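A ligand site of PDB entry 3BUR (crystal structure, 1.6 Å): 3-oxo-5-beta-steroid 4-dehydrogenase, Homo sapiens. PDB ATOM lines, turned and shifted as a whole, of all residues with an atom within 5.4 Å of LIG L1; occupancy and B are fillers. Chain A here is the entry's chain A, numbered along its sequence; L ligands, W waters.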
ATOM      1  N   TYR A  26      24.092  31.048   1.678  1.00  0.00           N
ATOM      2  CA  TYR A  26      23.134  29.995   1.966  1.00  0.00           C
ATOM      3  C   TYR A  26      23.377  29.580   3.428  1.00  0.00           C
ATOM      4  O   TYR A  26      24.496  29.314   3.835  1.00  0.00           O
ATOM      5  CB  TYR A  26      23.229  28.750   1.068  1.00  0.00           C
ATOM      6  CG  TYR A  26      22.358  27.627   1.625  1.00  0.00           C
ATOM      7  CD1 TYR A  26      20.980  27.656   1.428  1.00  0.00           C
ATOM      8  CD2 TYR A  26      22.882  26.543   2.340  1.00  0.00           C
ATOM      9  CE1 TYR A  26      20.214  26.626   1.943  1.00  0.00           C
ATOM     10  CE2 TYR A  26      22.111  25.525   2.861  1.00  0.00           C
ATOM     11  CZ  TYR A  26      20.755  25.581   2.649  1.00  0.00           C
ATOM     12  OH  TYR A  26      19.988  24.572   3.153  1.00  0.00           O
ATOM     13  N   ILE A  57      15.593  32.156  -2.776  1.00  0.00           N
ATOM     14  CA  ILE A  57      15.175  30.905  -2.156  1.00  0.00           C
ATOM     15  C   ILE A  57      16.030  30.564  -0.929  1.00  0.00           C
ATOM     16  O   ILE A  57      15.668  29.615  -0.216  1.00  0.00           O
ATOM     17  CB  ILE A  57      15.243  29.736  -3.145  1.00  0.00           C
ATOM     18  CG1 ILE A  57      16.629  29.348  -3.638  1.00  0.00           C
ATOM     19  CG2 ILE A  57      14.319  30.040  -4.325  1.00  0.00           C
ATOM     20  CD1 ILE A  57      16.754  27.868  -3.986  1.00  0.00           C
ATOM     21  N   TYR A  58      17.112  31.300  -0.672  1.00  0.00           N
ATOM     22  CA  TYR A  58      17.855  31.050   0.563  1.00  0.00           C
ATOM     23  C   TYR A  58      17.084  31.617   1.741  1.00  0.00           C
ATOM     24  O   TYR A  58      17.465  31.360   2.889  1.00  0.00           O
ATOM     25  CB  TYR A  58      19.267  31.631   0.571  1.00  0.00           C
ATOM     26  CG  TYR A  58      20.165  31.137  -0.539  1.00  0.00           C
ATOM     27  CD1 TYR A  58      19.815  30.059  -1.334  1.00  0.00           C
ATOM     28  CD2 TYR A  58      21.382  31.765  -0.801  1.00  0.00           C
ATOM     29  CE1 TYR A  58      20.631  29.591  -2.363  1.00  0.00           C
ATOM     30  CE2 TYR A  58      22.187  31.296  -1.821  1.00  0.00           C
ATOM     31  CZ  TYR A  58      21.820  30.229  -2.601  1.00  0.00           C
ATOM     32  OH  TYR A  58      22.657  29.804  -3.613  1.00  0.00           O
ATOM     33  N   TRP A  89      15.171  30.925  -9.598  1.00  0.00           N
ATOM     34  CA  TRP A  89      14.986  29.502  -9.245  1.00  0.00           C
ATOM     35  C   TRP A  89      14.120  28.780 -10.274  1.00  0.00           C
ATOM     36  O   TRP A  89      13.374  29.430 -11.017  1.00  0.00           O
ATOM     37  CB  TRP A  89      14.385  29.419  -7.837  1.00  0.00           C
ATOM     38  CG  TRP A  89      14.092  28.015  -7.412  1.00  0.00           C
ATOM     39  CD1 TRP A  89      12.876  27.536  -7.005  1.00  0.00           C
ATOM     40  CD2 TRP A  89      15.015  26.918  -7.355  1.00  0.00           C
ATOM     41  NE1 TRP A  89      13.001  26.196  -6.695  1.00  0.00           N
ATOM     42  CE2 TRP A  89      14.291  25.794  -6.886  1.00  0.00           C
ATOM     43  CE3 TRP A  89      16.374  26.774  -7.629  1.00  0.00           C
ATOM     44  CZ2 TRP A  89      14.898  24.541  -6.712  1.00  0.00           C
ATOM     45  CZ3 TRP A  89      16.986  25.533  -7.458  1.00  0.00           C
ATOM     46  CH2 TRP A  89      16.233  24.443  -6.999  1.00  0.00           C
ATOM     47  N   GLU A 120      19.332  29.703 -11.900  1.00  0.00           N
ATOM     48  CA  GLU A 120      19.873  29.019 -10.724  1.00  0.00           C
ATOM     49  C   GLU A 120      20.252  27.549 -10.968  1.00  0.00           C
ATOM     50  O   GLU A 120      21.272  27.030 -10.483  1.00  0.00           O
ATOM     51  CB  GLU A 120      18.859  29.082  -9.571  1.00  0.00           C
ATOM     52  CG  GLU A 120      19.490  28.714  -8.216  1.00  0.00           C
ATOM     53  CD  GLU A 120      18.760  29.399  -7.066  1.00  0.00           C
ATOM     54  OE1 GLU A 120      17.650  29.941  -7.250  1.00  0.00           O
ATOM     55  OE2 GLU A 120      19.280  29.401  -5.939  1.00  0.00           O
ATOM     56  N   VAL A 121      19.402  26.860 -11.693  1.00  0.00           N
ATOM     57  CA  VAL A 121      19.631  25.546 -12.264  1.00  0.00           C
ATOM     58  C   VAL A 121      19.038  25.501 -13.677  1.00  0.00           C
ATOM     59  O   VAL A 121      18.115  26.274 -13.971  1.00  0.00           O
ATOM     60  CB  VAL A 121      19.002  24.450 -11.408  1.00  0.00           C
ATOM     61  CG1 VAL A 121      19.792  24.291 -10.110  1.00  0.00           C
ATOM     62  CG2 VAL A 121      17.527  24.721 -11.118  1.00  0.00           C
ATOM     63  N   ILE A 131       9.085  25.972  -3.404  1.00  0.00           N
ATOM     64  CA  ILE A 131      10.419  25.894  -3.985  1.00  0.00           C
ATOM     65  C   ILE A 131      10.685  24.483  -4.500  1.00  0.00           C
ATOM     66  O   ILE A 131      11.286  24.295  -5.549  1.00  0.00           O
ATOM     67  CB  ILE A 131      11.482  26.301  -2.949  1.00  0.00           C
ATOM     68  CG1 ILE A 131      11.407  27.790  -2.574  1.00  0.00           C
ATOM     69  CG2 ILE A 131      12.893  25.935  -3.378  1.00  0.00           C
ATOM     70  CD1 ILE A 131      11.665  28.008  -1.091  1.00  0.00           C
ATOM     71  N   TYR A 132      10.246  23.458  -3.753  1.00  0.00           N
ATOM     72  CA  TYR A 132      10.502  22.085  -4.200  1.00  0.00           C
ATOM     73  C   TYR A 132       9.171  21.338  -4.313  1.00  0.00           C
ATOM     74  O   TYR A 132       8.805  20.613  -3.388  1.00  0.00           O
ATOM     75  CB  TYR A 132      11.444  21.373  -3.243  1.00  0.00           C
ATOM     76  CG  TYR A 132      12.679  22.158  -2.845  1.00  0.00           C
ATOM     77  CD1 TYR A 132      12.723  22.865  -1.647  1.00  0.00           C
ATOM     78  CD2 TYR A 132      13.803  22.208  -3.651  1.00  0.00           C
ATOM     79  CE1 TYR A 132      13.840  23.586  -1.262  1.00  0.00           C
ATOM     80  CE2 TYR A 132      14.927  22.923  -3.281  1.00  0.00           C
ATOM     81  CZ  TYR A 132      14.943  23.618  -2.083  1.00  0.00           C
ATOM     82  OH  TYR A 132      16.056  24.332  -1.704  1.00  0.00           O
ATOM     83  N   TYR A 219      30.973  27.792  -6.577  1.00  0.00           N
ATOM     84  CA  TYR A 219      30.173  27.617  -5.369  1.00  0.00           C
ATOM     85  C   TYR A 219      30.775  26.450  -4.569  1.00  0.00           C
ATOM     86  O   TYR A 219      31.582  25.697  -5.120  1.00  0.00           O
ATOM     87  CB  TYR A 219      28.705  27.442  -5.679  1.00  0.00           C
ATOM     88  CG  TYR A 219      28.011  26.219  -6.180  1.00  0.00           C
ATOM     89  CD1 TYR A 219      27.985  24.999  -5.512  1.00  0.00           C
ATOM     90  CD2 TYR A 219      27.295  26.235  -7.382  1.00  0.00           C
ATOM     91  CE1 TYR A 219      27.336  23.869  -5.973  1.00  0.00           C
ATOM     92  CE2 TYR A 219      26.621  25.125  -7.871  1.00  0.00           C
ATOM     93  CZ  TYR A 219      26.647  23.941  -7.160  1.00  0.00           C
ATOM     94  OH  TYR A 219      25.990  22.813  -7.598  1.00  0.00           O
ATOM     95  N   SER A 220      30.350  26.320  -3.319  1.00  0.00           N
ATOM     96  CA  SER A 220      30.938  25.363  -2.375  1.00  0.00           C
ATOM     97  C   SER A 220      32.457  25.259  -2.500  1.00  0.00           C
ATOM     98  O   SER A 220      32.998  24.148  -2.620  1.00  0.00           O
ATOM     99  CB  SER A 220      30.269  24.006  -2.585  1.00  0.00           C
ATOM    100  OG  SER A 220      28.862  24.136  -2.446  1.00  0.00           O
ATOM    101  N   THR A 224      31.490  22.433   0.745  1.00  0.00           N
ATOM    102  CA  THR A 224      30.152  22.431   1.313  1.00  0.00           C
ATOM    103  C   THR A 224      30.163  22.270   2.843  1.00  0.00           C
ATOM    104  O   THR A 224      31.147  21.892   3.475  1.00  0.00           O
ATOM    105  CB  THR A 224      29.156  21.369   0.800  1.00  0.00           C
ATOM    106  OG1 THR A 224      29.432  20.076   1.390  1.00  0.00           O
ATOM    107  CG2 THR A 224      29.229  21.133  -0.711  1.00  0.00           C
ATOM    108  N   SER A 225      28.984  22.572   3.386  1.00  0.00           N
ATOM    109  CA  SER A 225      28.721  22.336   4.806  1.00  0.00           C
ATOM    110  C   SER A 225      28.459  20.854   5.074  1.00  0.00           C
ATOM    111  O   SER A 225      28.268  20.432   6.212  1.00  0.00           O
ATOM    112  CB  SER A 225      27.533  23.187   5.246  1.00  0.00           C
ATOM    113  OG  SER A 225      26.346  22.654   4.675  1.00  0.00           O
ATOM    114  N   ARG A 226      28.462  20.032   4.029  1.00  0.00           N
ATOM    115  CA  ARG A 226      28.316  18.592   4.110  1.00  0.00           C
ATOM    116  C   ARG A 226      27.009  18.167   4.754  1.00  0.00           C
ATOM    117  O   ARG A 226      26.938  17.236   5.571  1.00  0.00           O
ATOM    118  CB  ARG A 226      29.539  17.997   4.862  1.00  0.00           C
ATOM    119  CG  ARG A 226      30.841  18.393   4.187  1.00  0.00           C
ATOM    120  CD  ARG A 226      32.068  17.795   4.844  1.00  0.00           C
ATOM    121  NE  ARG A 226      31.983  16.341   4.940  1.00  0.00           N
ATOM    122  CZ  ARG A 226      32.362  15.481   4.018  1.00  0.00           C
ATOM    123  NH1 ARG A 226      32.873  15.884   2.862  1.00  0.00           N
ATOM    124  NH2 ARG A 226      32.228  14.167   4.233  1.00  0.00           N
ATOM    125  N   ASN A 227      25.904  18.819   4.388  1.00  0.00           N
ATOM    126  CA  ASN A 227      24.600  18.308   4.830  1.00  0.00           C
ATOM    127  C   ASN A 227      24.280  16.997   4.105  1.00  0.00           C
ATOM    128  O   ASN A 227      24.365  16.962   2.867  1.00  0.00           O
ATOM    129  CB  ASN A 227      23.514  19.346   4.576  1.00  0.00           C
ATOM    130  CG  ASN A 227      22.168  18.942   5.143  1.00  0.00           C
ATOM    131  OD1 ASN A 227      21.819  17.763   5.184  1.00  0.00           O
ATOM    132  ND2 ASN A 227      21.417  19.956   5.577  1.00  0.00           N
ATOM    133  N   TRP A 230      22.223  16.695   0.771  1.00  0.00           N
ATOM    134  CA  TRP A 230      22.784  17.058  -0.516  1.00  0.00           C
ATOM    135  C   TRP A 230      24.169  16.519  -0.828  1.00  0.00           C
ATOM    136  O   TRP A 230      24.517  16.401  -2.004  1.00  0.00           O
ATOM    137  CB  TRP A 230      22.880  18.603  -0.580  1.00  0.00           C
ATOM    138  CG  TRP A 230      21.590  19.237  -0.170  1.00  0.00           C
ATOM    139  CD1 TRP A 230      21.136  19.649   1.039  1.00  0.00           C
ATOM    140  CD2 TRP A 230      20.551  19.542  -1.114  1.00  0.00           C
ATOM    141  NE1 TRP A 230      19.868  20.193   0.930  1.00  0.00           N
ATOM    142  CE2 TRP A 230      19.494  20.132  -0.390  1.00  0.00           C
ATOM    143  CE3 TRP A 230      20.461  19.340  -2.497  1.00  0.00           C
ATOM    144  CZ2 TRP A 230      18.331  20.530  -1.034  1.00  0.00           C
ATOM    145  CZ3 TRP A 230      19.291  19.745  -3.126  1.00  0.00           C
ATOM    146  CH2 TRP A 230      18.258  20.336  -2.384  1.00  0.00           C
ATOM    147  N   VAL A 231      24.948  16.189   0.191  1.00  0.00           N
ATOM    148  CA  VAL A 231      26.310  15.695   0.042  1.00  0.00           C
ATOM    149  C   VAL A 231      26.466  14.273   0.546  1.00  0.00           C
ATOM    150  O   VAL A 231      25.842  13.937   1.554  1.00  0.00           O
ATOM    151  CB  VAL A 231      27.279  16.584   0.848  1.00  0.00           C
ATOM    152  CG1 VAL A 231      28.710  16.098   0.694  1.00  0.00           C
ATOM    153  CG2 VAL A 231      27.131  18.018   0.378  1.00  0.00           C
ATOM    154  N   VAL A 309      28.206  17.722  -4.850  1.00  0.00           N
ATOM    155  CA  VAL A 309      26.808  18.066  -5.031  1.00  0.00           C
ATOM    156  C   VAL A 309      26.307  17.432  -6.323  1.00  0.00           C
ATOM    157  O   VAL A 309      26.505  17.983  -7.408  1.00  0.00           O
ATOM    158  CB  VAL A 309      26.621  19.594  -5.090  1.00  0.00           C
ATOM    159  CG1 VAL A 309      25.164  20.011  -5.181  1.00  0.00           C
ATOM    160  CG2 VAL A 309      27.266  20.236  -3.858  1.00  0.00           C
ATOM    161  N   LEU A 311      23.080  16.379  -6.815  1.00  0.00           N
ATOM    162  CA  LEU A 311      21.677  16.698  -7.070  1.00  0.00           C
ATOM    163  C   LEU A 311      20.920  15.448  -7.505  1.00  0.00           C
ATOM    164  O   LEU A 311      20.052  15.514  -8.379  1.00  0.00           O
ATOM    165  CB  LEU A 311      21.594  17.789  -8.141  1.00  0.00           C
ATOM    166  CG  LEU A 311      21.419  19.243  -7.700  1.00  0.00           C
ATOM    167  CD1 LEU A 311      21.956  19.478  -6.293  1.00  0.00           C
ATOM    168  CD2 LEU A 311      22.078  20.186  -8.699  1.00  0.00           C
ATOM    169  N   TRP A 314      17.214  14.843  -8.816  1.00  0.00           N
ATOM    170  CA  TRP A 314      16.668  15.474 -10.024  1.00  0.00           C
ATOM    171  C   TRP A 314      17.286  14.897 -11.285  1.00  0.00           C
ATOM    172  O   TRP A 314      17.246  15.437 -12.388  1.00  0.00           O
ATOM    173  CB  TRP A 314      16.874  16.994  -9.940  1.00  0.00           C
ATOM    174  CG  TRP A 314      16.172  17.618  -8.761  1.00  0.00           C
ATOM    175  CD1 TRP A 314      14.987  17.253  -8.198  1.00  0.00           C
ATOM    176  CD2 TRP A 314      16.630  18.743  -8.000  1.00  0.00           C
ATOM    177  NE1 TRP A 314      14.685  18.068  -7.134  1.00  0.00           N
ATOM    178  CE2 TRP A 314      15.680  18.994  -6.995  1.00  0.00           C
ATOM    179  CE3 TRP A 314      17.776  19.551  -8.088  1.00  0.00           C
ATOM    180  CZ2 TRP A 314      15.789  20.026  -6.052  1.00  0.00           C
ATOM    181  CZ3 TRP A 314      17.889  20.572  -7.151  1.00  0.00           C
ATOM    182  CH2 TRP A 314      16.924  20.792  -6.167  1.00  0.00           C
HETATM  183  C1  LIG L   1      22.869  22.545   1.208  1.00  0.00           C
HETATM  184  C2  LIG L   1      24.042  22.316   2.153  1.00  0.00           C
HETATM  185  C3  LIG L   1      25.047  21.406   1.513  1.00  0.00           C
HETATM  186  O1  LIG L   1      25.794  20.715   2.220  1.00  0.00           O
HETATM  187  C4  LIG L   1      25.317  21.634   0.101  1.00  0.00           C
HETATM  188  C5  LIG L   1      24.388  22.189  -0.734  1.00  0.00           C
HETATM  189  C6  LIG L   1      24.643  22.244  -2.191  1.00  0.00           C
HETATM  190  C7  LIG L   1      23.390  22.316  -3.078  1.00  0.00           C
HETATM  191  C8  LIG L   1      22.396  23.370  -2.599  1.00  0.00           C
HETATM  192  C9  LIG L   1      22.053  23.091  -1.114  1.00  0.00           C
HETATM  193  C10 LIG L   1      23.296  23.111  -0.163  1.00  0.00           C
HETATM  194  C11 LIG L   1      20.912  24.012  -0.601  1.00  0.00           C
HETATM  195  C12 LIG L   1      19.647  23.912  -1.497  1.00  0.00           C
HETATM  196  C13 LIG L   1      20.027  24.265  -2.944  1.00  0.00           C
HETATM  197  C14 LIG L   1      21.102  23.266  -3.410  1.00  0.00           C
HETATM  198  C15 LIG L   1      21.164  23.443  -4.940  1.00  0.00           C
HETATM  199  C16 LIG L   1      19.746  23.873  -5.345  1.00  0.00           C
HETATM  200  C17 LIG L   1      18.935  23.943  -4.007  1.00  0.00           C
HETATM  201  O2  LIG L   1      17.922  24.948  -4.112  1.00  0.00           O
HETATM  202  C18 LIG L   1      20.404  25.735  -3.067  1.00  0.00           C
HETATM  203  C19 LIG L   1      23.914  24.515  -0.042  1.00  0.00           C
HETATM  204  P1  LG2 L   2      31.237  26.259   1.253  1.00  0.00           P
HETATM  205  O1  LG2 L   2      32.071  25.457   0.466  1.00  0.00           O
HETATM  206  O2  LG2 L   2      31.385  27.754   1.146  1.00  0.00           O
HETATM  207  O3  LG2 L   2      31.397  25.859   2.849  1.00  0.00           O
HETATM  208  C1  LG2 L   2      30.780  26.384   3.822  1.00  0.00           C
HETATM  209  C2  LG2 L   2      30.834  25.554   5.145  1.00  0.00           C
HETATM  210  O4  LG2 L   2      32.123  25.800   5.580  1.00  0.00           O
HETATM  211  C3  LG2 L   2      29.947  26.139   6.288  1.00  0.00           C
HETATM  212  O5  LG2 L   2      29.539  25.031   7.075  1.00  0.00           O
HETATM  213  C4  LG2 L   2      30.876  27.065   7.049  1.00  0.00           C
HETATM  214  O6  LG2 L   2      30.566  27.158   8.464  1.00  0.00           O
HETATM  215  C5  LG2 L   2      32.217  26.385   6.881  1.00  0.00           C
HETATM  216  N1  LG2 L   2      33.371  27.257   6.808  1.00  0.00           N
HETATM  217  C6  LG2 L   2      33.443  28.492   6.217  1.00  0.00           C
HETATM  218  N2  LG2 L   2      34.709  28.989   6.265  1.00  0.00           N
HETATM  219  C7  LG2 L   2      35.410  28.012   6.925  1.00  0.00           C
HETATM  220  C8  LG2 L   2      36.764  28.027   7.284  1.00  0.00           C
HETATM  221  N3  LG2 L   2      37.690  28.946   7.100  1.00  0.00           N
HETATM  222  N4  LG2 L   2      37.226  26.836   7.971  1.00  0.00           N
HETATM  223  C9  LG2 L   2      36.383  25.799   8.209  1.00  0.00           C
HETATM  224  N5  LG2 L   2      35.076  25.807   7.896  1.00  0.00           N
HETATM  225  C10 LG2 L   2      34.564  26.960   7.223  1.00  0.00           C
HETATM  226  O7  LG2 L   2      29.749  26.050   0.871  1.00  0.00           O
HETATM  227  P2  LG2 L   2      28.406  26.471   0.347  1.00  0.00           P
HETATM  228  O8  LG2 L   2      27.668  25.380  -0.085  1.00  0.00           O
HETATM  229  O9  LG2 L   2      27.792  27.432   1.352  1.00  0.00           O
HETATM  230  O10 LG2 L   2      28.978  27.283  -0.723  1.00  0.00           O
HETATM  231  C11 LG2 L   2      29.197  28.662  -0.942  1.00  0.00           C
HETATM  232  C12 LG2 L   2      28.121  29.564  -1.426  1.00  0.00           C
HETATM  233  O11 LG2 L   2      27.909  29.269  -2.851  1.00  0.00           O
HETATM  234  C13 LG2 L   2      26.677  29.351  -0.837  1.00  0.00           C
HETATM  235  O12 LG2 L   2      26.516  29.926   0.513  1.00  0.00           O
HETATM  236  C14 LG2 L   2      25.812  29.969  -1.963  1.00  0.00           C
HETATM  237  O13 LG2 L   2      25.932  31.414  -1.822  1.00  0.00           O
HETATM  238  C15 LG2 L   2      26.529  29.437  -3.191  1.00  0.00           C
HETATM  239  N6  LG2 L   2      26.071  28.105  -3.708  1.00  0.00           N
HETATM  240  C16 LG2 L   2      25.412  28.152  -4.939  1.00  0.00           C
HETATM  241  C17 LG2 L   2      24.733  27.001  -5.384  1.00  0.00           C
HETATM  242  C18 LG2 L   2      24.020  27.068  -6.719  1.00  0.00           C
HETATM  243  O14 LG2 L   2      23.435  26.065  -7.105  1.00  0.00           O
HETATM  244  N7  LG2 L   2      24.109  28.249  -7.339  1.00  0.00           N
HETATM  245  C19 LG2 L   2      24.718  25.790  -4.602  1.00  0.00           C
HETATM  246  C20 LG2 L   2      25.391  25.719  -3.347  1.00  0.00           C
HETATM  247  C21 LG2 L   2      26.057  26.867  -2.907  1.00  0.00           C
HETATM  248  P3  LG2 L   2      30.502  28.617   9.200  1.00  0.00           P
HETATM  249  O15 LG2 L   2      29.403  29.446   8.551  1.00  0.00           O
HETATM  250  O16 LG2 L   2      30.130  28.280  10.657  1.00  0.00           O
HETATM  251  O17 LG2 L   2      31.883  29.254   9.035  1.00  0.00           O
HETATM  252  O   HOH W   1      21.456  28.180  -5.283  1.00  0.00           O
HETATM  253  O   HOH W   2      26.989  23.910   1.870  1.00  0.00           O
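N of Arg 226 is in hydrogen-bond range of OG1 of Thr 224, 2.8 Å away. The indole nitrogen (NE1) of Trp 89 is in hydrogen-bond range of the backbone carbonyl oxygen (O) of Ile 131 (2.8 Å).
O1 of LIG L1 is in hydrogen-bond range of N of Arg 226 (3.3 Å). The side-chain hydroxyl (OG) of Ser 225 is in hydrogen-bond range of an oxygen (O1) of LIG L1, 3.2 Å away. The backbone NH of Asn 227 lies within hydrogen-bond range of an oxygen (O1) of LIG L1 (2.9 Å). The side-chain hydroxyl of Tyr 132 sits at hydrogen-bond distance from an oxygen (O2) of LIG L1, 3.1 Å away. The side-chain hydroxyl of Ser 220 lies within hydrogen-bond range of an oxygen (O8) of LG2 L2. N of Tyr 26 lies within hydrogen-bond range of O12 of LG2 L2 (2.9 Å). N of Thr 224 sits at hydrogen-bond distance from O1 of LG2 L2 (3.1 Å). The backbone NH (N) of Ser 220 lies within hydrogen-bond range of an oxygen (O10) of LG2 L2, 3.1 Å away.
Residues that only touch LIG L1: Ile 57 (3.1 Å), Tyr 26 (3.3 Å), Trp 230 (3.4 Å), Trp 89 (3.4 Å), Val 231 (3.5 Å), Val 309 (3.6 Å), Thr 224 (3.7 Å) and Tyr 58 (3.9 Å). Of the 19 residues printed, 12 come within 4 Å of LIG L1. The nearest printed residue that does not touch LIG L1 is Trp 314 (4.2 Å).
Water W2 lies within hydrogen-bond range of an oxygen (O8) of LG2 L2 (2.5 Å), the backbone NH (N) of Ser 225 (2.8 Å) and an oxygen (O1) of LIG L1 (3.4 Å). Water W1 lies within hydrogen-bond range of OE2 of Glu 120 (2.6 Å), OH of Tyr 58 (2.6 Å) and N7 of LG2 L2 (3.4 Å).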
